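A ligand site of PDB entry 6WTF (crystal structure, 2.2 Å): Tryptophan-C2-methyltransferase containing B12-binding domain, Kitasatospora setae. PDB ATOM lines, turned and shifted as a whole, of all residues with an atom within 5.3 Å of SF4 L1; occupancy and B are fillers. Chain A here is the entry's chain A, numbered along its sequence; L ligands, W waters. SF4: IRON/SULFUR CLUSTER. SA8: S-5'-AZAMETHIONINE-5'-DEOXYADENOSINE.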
ATOM      1  N   CYS A 227      -2.784  -1.649   1.861  1.00  0.00           N
ATOM      2  CA  CYS A 227      -2.570  -1.517   0.424  1.00  0.00           C
ATOM      3  C   CYS A 227      -1.478  -0.496   0.184  1.00  0.00           C
ATOM      4  O   CYS A 227      -1.559   0.625   0.684  1.00  0.00           O
ATOM      5  CB  CYS A 227      -3.854  -1.102  -0.306  1.00  0.00           C
ATOM      6  SG  CYS A 227      -3.660  -1.051  -2.107  1.00  0.00           S
ATOM      7  N   TYR A 229      -0.700   0.968  -2.628  1.00  0.00           N
ATOM      8  CA  TYR A 229      -0.937   1.936  -3.691  1.00  0.00           C
ATOM      9  C   TYR A 229      -1.641   3.159  -3.122  1.00  0.00           C
ATOM     10  O   TYR A 229      -1.767   3.336  -1.906  1.00  0.00           O
ATOM     11  CB  TYR A 229      -1.723   1.294  -4.840  1.00  0.00           C
ATOM     12  CG  TYR A 229      -0.900   0.327  -5.651  1.00  0.00           C
ATOM     13  CD1 TYR A 229       0.471   0.204  -5.453  1.00  0.00           C
ATOM     14  CD2 TYR A 229      -1.492  -0.473  -6.620  1.00  0.00           C
ATOM     15  CE1 TYR A 229       1.232  -0.687  -6.200  1.00  0.00           C
ATOM     16  CE2 TYR A 229      -0.739  -1.361  -7.370  1.00  0.00           C
ATOM     17  CZ  TYR A 229       0.613  -1.458  -7.155  1.00  0.00           C
ATOM     18  OH  TYR A 229       1.365  -2.341  -7.896  1.00  0.00           O
ATOM     19  N   ARG A 230      -2.121   4.030  -4.006  1.00  0.00           N
ATOM     20  CA  ARG A 230      -2.631   5.327  -3.578  1.00  0.00           C
ATOM     21  C   ARG A 230      -3.673   5.808  -4.575  1.00  0.00           C
ATOM     22  O   ARG A 230      -3.675   6.959  -4.998  1.00  0.00           O
ATOM     23  CB  ARG A 230      -1.485   6.325  -3.424  1.00  0.00           C
ATOM     24  CG  ARG A 230      -1.799   7.521  -2.547  1.00  0.00           C
ATOM     25  CD  ARG A 230      -2.098   7.108  -1.096  1.00  0.00           C
ATOM     26  NE  ARG A 230      -0.935   6.568  -0.408  1.00  0.00           N
ATOM     27  CZ  ARG A 230      -0.076   7.292   0.300  1.00  0.00           C
ATOM     28  NH1 ARG A 230      -0.256   8.604   0.418  1.00  0.00           N
ATOM     29  NH2 ARG A 230       0.955   6.720   0.904  1.00  0.00           N
ATOM     30  N   CYS A 231      -4.593   4.920  -4.968  1.00  0.00           N
ATOM     31  CA  CYS A 231      -5.613   5.287  -5.942  1.00  0.00           C
ATOM     32  C   CYS A 231      -6.461   6.423  -5.406  1.00  0.00           C
ATOM     33  O   CYS A 231      -6.950   6.370  -4.270  1.00  0.00           O
ATOM     34  CB  CYS A 231      -6.465   4.072  -6.289  1.00  0.00           C
ATOM     35  SG  CYS A 231      -5.517   2.685  -6.981  1.00  0.00           S
ATOM     36  N   HIS A 233      -9.322   7.517  -5.512  1.00  0.00           N
ATOM     37  CA  HIS A 233     -10.700   7.356  -5.079  1.00  0.00           C
ATOM     38  C   HIS A 233     -10.825   6.578  -3.771  1.00  0.00           C
ATOM     39  O   HIS A 233     -11.912   6.590  -3.171  1.00  0.00           O
ATOM     40  CB  HIS A 233     -11.490   6.608  -6.163  1.00  0.00           C
ATOM     41  CG  HIS A 233     -11.130   5.155  -6.276  1.00  0.00           C
ATOM     42  ND1 HIS A 233     -10.036   4.716  -6.996  1.00  0.00           N
ATOM     43  CD2 HIS A 233     -11.690   4.050  -5.739  1.00  0.00           C
ATOM     44  CE1 HIS A 233      -9.959   3.406  -6.911  1.00  0.00           C
ATOM     45  NE2 HIS A 233     -10.946   2.974  -6.152  1.00  0.00           N
ATOM     46  N   CYS A 234      -9.775   5.920  -3.314  1.00  0.00           N
ATOM     47  CA  CYS A 234      -9.895   4.800  -2.376  1.00  0.00           C
ATOM     48  C   CYS A 234      -9.452   5.209  -0.980  1.00  0.00           C
ATOM     49  O   CYS A 234      -8.348   5.747  -0.802  1.00  0.00           O
ATOM     50  CB  CYS A 234      -9.067   3.614  -2.863  1.00  0.00           C
ATOM     51  SG  CYS A 234      -9.472   2.069  -2.042  1.00  0.00           S
ATOM     52  N   GLU A 236      -8.785   3.039   1.419  1.00  0.00           N
ATOM     53  CA  GLU A 236      -8.136   1.926   2.108  1.00  0.00           C
ATOM     54  C   GLU A 236      -6.673   2.153   2.439  1.00  0.00           C
ATOM     55  O   GLU A 236      -6.234   1.768   3.536  1.00  0.00           O
ATOM     56  CB  GLU A 236      -8.290   0.615   1.308  1.00  0.00           C
ATOM     57  CG  GLU A 236      -9.735   0.227   1.070  1.00  0.00           C
ATOM     58  CD  GLU A 236      -9.891  -1.194   0.562  1.00  0.00           C
ATOM     59  OE1 GLU A 236      -9.036  -2.049   0.877  1.00  0.00           O
ATOM     60  OE2 GLU A 236     -10.861  -1.458  -0.168  1.00  0.00           O
ATOM     61  N   PRO A 237      -5.845   2.741   1.555  1.00  0.00           N
ATOM     62  CA  PRO A 237      -4.444   2.978   1.938  1.00  0.00           C
ATOM     63  C   PRO A 237      -4.303   3.730   3.247  1.00  0.00           C
ATOM     64  O   PRO A 237      -3.467   3.376   4.087  1.00  0.00           O
ATOM     65  CB  PRO A 237      -3.885   3.771   0.760  1.00  0.00           C
ATOM     66  CG  PRO A 237      -4.706   3.377  -0.374  1.00  0.00           C
ATOM     67  CD  PRO A 237      -6.081   3.117   0.144  1.00  0.00           C
ATOM     68  N   SER A 272      -7.296  -5.834   0.733  1.00  0.00           N
ATOM     69  CA  SER A 272      -7.516  -4.711  -0.169  1.00  0.00           C
ATOM     70  C   SER A 272      -7.526  -5.184  -1.612  1.00  0.00           C
ATOM     71  O   SER A 272      -8.456  -4.887  -2.367  1.00  0.00           O
ATOM     72  CB  SER A 272      -6.446  -3.641   0.051  1.00  0.00           C
ATOM     73  OG  SER A 272      -6.659  -2.969   1.282  1.00  0.00           O
ATOM     74  N   GLU A 273      -6.505  -5.938  -2.006  1.00  0.00           N
ATOM     75  CA  GLU A 273      -6.443  -6.594  -3.310  1.00  0.00           C
ATOM     76  C   GLU A 273      -5.705  -7.906  -3.128  1.00  0.00           C
ATOM     77  O   GLU A 273      -4.572  -7.915  -2.645  1.00  0.00           O
ATOM     78  CB  GLU A 273      -5.719  -5.724  -4.346  1.00  0.00           C
ATOM     79  CG  GLU A 273      -6.257  -4.323  -4.518  1.00  0.00           C
ATOM     80  CD  GLU A 273      -7.599  -4.271  -5.221  1.00  0.00           C
ATOM     81  OE1 GLU A 273      -8.036  -5.297  -5.778  1.00  0.00           O
ATOM     82  OE2 GLU A 273      -8.211  -3.194  -5.222  1.00  0.00           O
ATOM     83  N   LEU A 276      -2.286  -8.244  -5.141  1.00  0.00           N
ATOM     84  CA  LEU A 276      -1.181  -7.388  -4.724  1.00  0.00           C
ATOM     85  C   LEU A 276      -0.411  -8.051  -3.600  1.00  0.00           C
ATOM     86  O   LEU A 276      -0.963  -8.794  -2.794  1.00  0.00           O
ATOM     87  CB  LEU A 276      -1.661  -6.001  -4.298  1.00  0.00           C
ATOM     88  CG  LEU A 276      -2.288  -5.174  -5.421  1.00  0.00           C
ATOM     89  CD1 LEU A 276      -2.612  -3.766  -4.924  1.00  0.00           C
ATOM     90  CD2 LEU A 276      -1.368  -5.120  -6.639  1.00  0.00           C
ATOM     91  N   GLN A 310      -6.703  -6.451  -8.777  1.00  0.00           N
ATOM     92  CA  GLN A 310      -6.389  -5.423  -9.747  1.00  0.00           C
ATOM     93  C   GLN A 310      -5.964  -6.099 -11.048  1.00  0.00           C
ATOM     94  O   GLN A 310      -5.584  -7.273 -11.041  1.00  0.00           O
ATOM     95  CB  GLN A 310      -5.288  -4.507  -9.225  1.00  0.00           C
ATOM     96  CG  GLN A 310      -5.774  -3.511  -8.201  1.00  0.00           C
ATOM     97  CD  GLN A 310      -6.759  -2.536  -8.787  1.00  0.00           C
ATOM     98  OE1 GLN A 310      -6.409  -1.693  -9.618  1.00  0.00           O
ATOM     99  NE2 GLN A 310      -8.012  -2.638  -8.363  1.00  0.00           N
ATOM    100  N   ASP A 335     -11.887  -0.330 -13.621  1.00  0.00           N
ATOM    101  CA  ASP A 335     -12.314   1.045 -13.343  1.00  0.00           C
ATOM    102  C   ASP A 335     -12.424   1.921 -14.591  1.00  0.00           C
ATOM    103  O   ASP A 335     -13.367   2.711 -14.702  1.00  0.00           O
ATOM    104  CB  ASP A 335     -11.411   1.677 -12.290  1.00  0.00           C
ATOM    105  CG  ASP A 335     -11.580   1.015 -10.921  1.00  0.00           C
ATOM    106  OD1 ASP A 335     -12.672   0.462 -10.677  1.00  0.00           O
ATOM    107  OD2 ASP A 335     -10.641   1.053 -10.101  1.00  0.00           O
ATOM    108  N   LYS A 346      -5.665   5.747 -10.932  1.00  0.00           N
ATOM    109  CA  LYS A 346      -5.268   4.405 -10.515  1.00  0.00           C
ATOM    110  C   LYS A 346      -3.744   4.333 -10.555  1.00  0.00           C
ATOM    111  O   LYS A 346      -3.140   3.935 -11.551  1.00  0.00           O
ATOM    112  CB  LYS A 346      -5.915   3.350 -11.400  1.00  0.00           C
ATOM    113  CG  LYS A 346      -7.434   3.387 -11.383  1.00  0.00           C
ATOM    114  CD  LYS A 346      -7.975   3.004 -10.020  1.00  0.00           C
ATOM    115  CE  LYS A 346      -7.556   1.584  -9.631  1.00  0.00           C
ATOM    116  NZ  LYS A 346      -8.242   0.567 -10.460  1.00  0.00           N
ATOM    117  N   TYR A 354      -0.137   1.302 -13.150  1.00  0.00           N
ATOM    118  CA  TYR A 354       0.428  -0.021 -12.959  1.00  0.00           C
ATOM    119  C   TYR A 354      -0.265  -1.098 -13.781  1.00  0.00           C
ATOM    120  O   TYR A 354       0.052  -2.285 -13.633  1.00  0.00           O
ATOM    121  CB  TYR A 354       0.405  -0.409 -11.470  1.00  0.00           C
ATOM    122  CG  TYR A 354      -0.958  -0.279 -10.802  1.00  0.00           C
ATOM    123  CD1 TYR A 354      -1.353   0.935 -10.230  1.00  0.00           C
ATOM    124  CD2 TYR A 354      -1.829  -1.357 -10.741  1.00  0.00           C
ATOM    125  CE1 TYR A 354      -2.590   1.059  -9.624  1.00  0.00           C
ATOM    126  CE2 TYR A 354      -3.066  -1.233 -10.135  1.00  0.00           C
ATOM    127  CZ  TYR A 354      -3.446  -0.028  -9.580  1.00  0.00           C
ATOM    128  OH  TYR A 354      -4.675   0.099  -8.963  1.00  0.00           O
HETATM  129 FE1  SF4 L   1      -6.206   0.994  -5.438  1.00  0.00          FE
HETATM  130 FE2  SF4 L   1      -5.463  -0.342  -3.163  1.00  0.00          FE
HETATM  131 FE3  SF4 L   1      -7.469  -1.326  -4.741  1.00  0.00          FE
HETATM  132 FE4  SF4 L   1      -7.884   0.928  -3.269  1.00  0.00          FE
HETATM  133  S1  SF4 L   1      -7.471  -1.153  -2.469  1.00  0.00           S
HETATM  134  S2  SF4 L   1      -8.456   0.590  -5.459  1.00  0.00           S
HETATM  135  S3  SF4 L   1      -5.831   1.900  -3.369  1.00  0.00           S
HETATM  136  S4  SF4 L   1      -5.273  -1.074  -5.309  1.00  0.00           S
HETATM  137  N   SA8 L   2     -10.622  -3.286  -2.152  1.00  0.00           N
HETATM  138  CA  SA8 L   2     -11.440  -2.537  -3.119  1.00  0.00           C
HETATM  139  C   SA8 L   2     -12.774  -2.145  -2.492  1.00  0.00           C
HETATM  140  O   SA8 L   2     -13.206  -1.002  -2.927  1.00  0.00           O
HETATM  141  OXT SA8 L   2     -13.352  -2.835  -1.677  1.00  0.00           O
HETATM  142  CB  SA8 L   2     -11.678  -3.347  -4.429  1.00  0.00           C
HETATM  143  CG  SA8 L   2     -11.899  -2.449  -5.639  1.00  0.00           C
HETATM  144  ND  SA8 L   2     -13.230  -1.840  -5.681  1.00  0.00           N
HETATM  145  CE  SA8 L   2     -14.269  -2.877  -5.737  1.00  0.00           C
HETATM  146  C5' SA8 L   2     -13.336  -0.835  -6.738  1.00  0.00           C
HETATM  147  C4' SA8 L   2     -14.723  -0.240  -6.860  1.00  0.00           C
HETATM  148  O4' SA8 L   2     -15.147   0.294  -5.579  1.00  0.00           O
HETATM  149  C3' SA8 L   2     -14.777   0.975  -7.782  1.00  0.00           C
HETATM  150  O3' SA8 L   2     -14.877   0.576  -9.149  1.00  0.00           O
HETATM  151  C2' SA8 L   2     -16.041   1.684  -7.297  1.00  0.00           C
HETATM  152  O2' SA8 L   2     -17.201   1.134  -7.904  1.00  0.00           O
HETATM  153  C1' SA8 L   2     -16.023   1.377  -5.789  1.00  0.00           C
HETATM  154  N9  SA8 L   2     -15.581   2.502  -4.957  1.00  0.00           N
HETATM  155  C8  SA8 L   2     -14.501   2.532  -4.122  1.00  0.00           C
HETATM  156  N7  SA8 L   2     -14.330   3.685  -3.515  1.00  0.00           N
HETATM  157  C5  SA8 L   2     -15.385   4.461  -3.972  1.00  0.00           C
HETATM  158  C6  SA8 L   2     -15.781   5.789  -3.707  1.00  0.00           C
HETATM  159  N6  SA8 L   2     -15.106   6.625  -2.908  1.00  0.00           N
HETATM  160  N1  SA8 L   2     -16.899   6.239  -4.314  1.00  0.00           N
HETATM  161  C2  SA8 L   2     -17.562   5.430  -5.145  1.00  0.00           C
HETATM  162  N3  SA8 L   2     -17.270   4.165  -5.488  1.00  0.00           N
HETATM  163  C4  SA8 L   2     -16.170   3.740  -4.864  1.00  0.00           C
HETATM  164  O   HOH W   1     -10.147  -0.791  -8.128  1.00  0.00           O
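A sulfur (S2) of SF4 L1 sits close to a ring nitrogen (NE2) of His 233 (3.5 Å).
The side-chain sulfur of Cys 231 binds an iron atom (FE1) of SF4 L1 (2.4 Å).
The backbone carbonyl oxygen (O) of Ser 272 sits at hydrogen-bond distance from a nitrogen (N) of SA8 L2, 2.7 Å away.
An iron atom (FE2) of SF4 L1 is bound by the side-chain sulfur (SG) of Cys 227 (2.2 Å).
A nitrogen (N) of SA8 L2 lies close to the side-chain carboxylate (OE2) of Glu 273 (3.9 Å).
The backbone NH (N) of Cys 231 lies close to a sulfur (S3) of SF4 L1, at 3.6 Å.
An iron atom (FE4) of SF4 L1 is bound by the side-chain sulfur (SG) of Cys 234 (2.3 Å).
A nitrogen (N6) of SA8 L2 lies within hydrogen-bond range of the backbone carbonyl oxygen of His 233 (3.2 Å).
The side-chain carboxylate (OD1) of Asp 335 is in hydrogen-bond range of an oxygen (O3') of SA8 L2.
OE2 of Glu 236 is in salt-bridge range of N of SA8 L2 (2.7 Å).
The side-chain carboxylate (OE2) of Glu 273 binds an iron atom (FE3) of SF4 L1 (2.1 Å).
SG of Cys 231 sits close to OH of Tyr 354 (3.4 Å).
N of Tyr 229 sits close to SG of Cys 227 (3.6 Å).
The side-chain sulfur (SG) of Cys 234 lies close to the backbone NH (N) of Glu 236 (3.7 Å).
OE1 of Glu 273 sits at hydrogen-bond distance from N of Gln 310, at 3.5 Å.
OE1 of Gln 310 lies within hydrogen-bond range of NZ of Lys 346 (3.0 Å).
The side-chain hydroxyl of Ser 272 is in hydrogen-bond range of the side-chain carboxylate of Glu 236, 2.6 Å away.
The side-chain amide oxygen (OE1) of Gln 310 lies within hydrogen-bond range of the side-chain hydroxyl (OH) of Tyr 354.
Glu 236 touches SF4 L1.
CG of Pro 237 touches S3 of SF4 L1 (3.5 Å).
Ser 272 touches SF4 L1.
Leu 276 touches SF4 L1 (CD1 to S4, 3.8 Å).
Gln 310 touches SF4 L1.
OH of Tyr 354 touches S4 of SF4 L1, 3.9 Å away.
Within 4 Å of SF4 L1: Cys 227, Cys 231, His 233, Cys 234, Glu 236, Pro 237, Ser 272, Glu 273, Leu 276, Gln 310 and Tyr 354.
Along chain A the residues within 4 Å of SF4 L1 span positions 227 to 354.
Water W1 lies within hydrogen-bond range of the side-chain carboxylate (OD2) of Asp 335 (2.7 Å), the side-chain amide nitrogen (NE2) of Gln 310 (2.8 Å), the side-chain amino group (NZ) of Lys 346 (3.3 Å) and a sulfur (S2) of SF4 L1 (3.4 Å).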
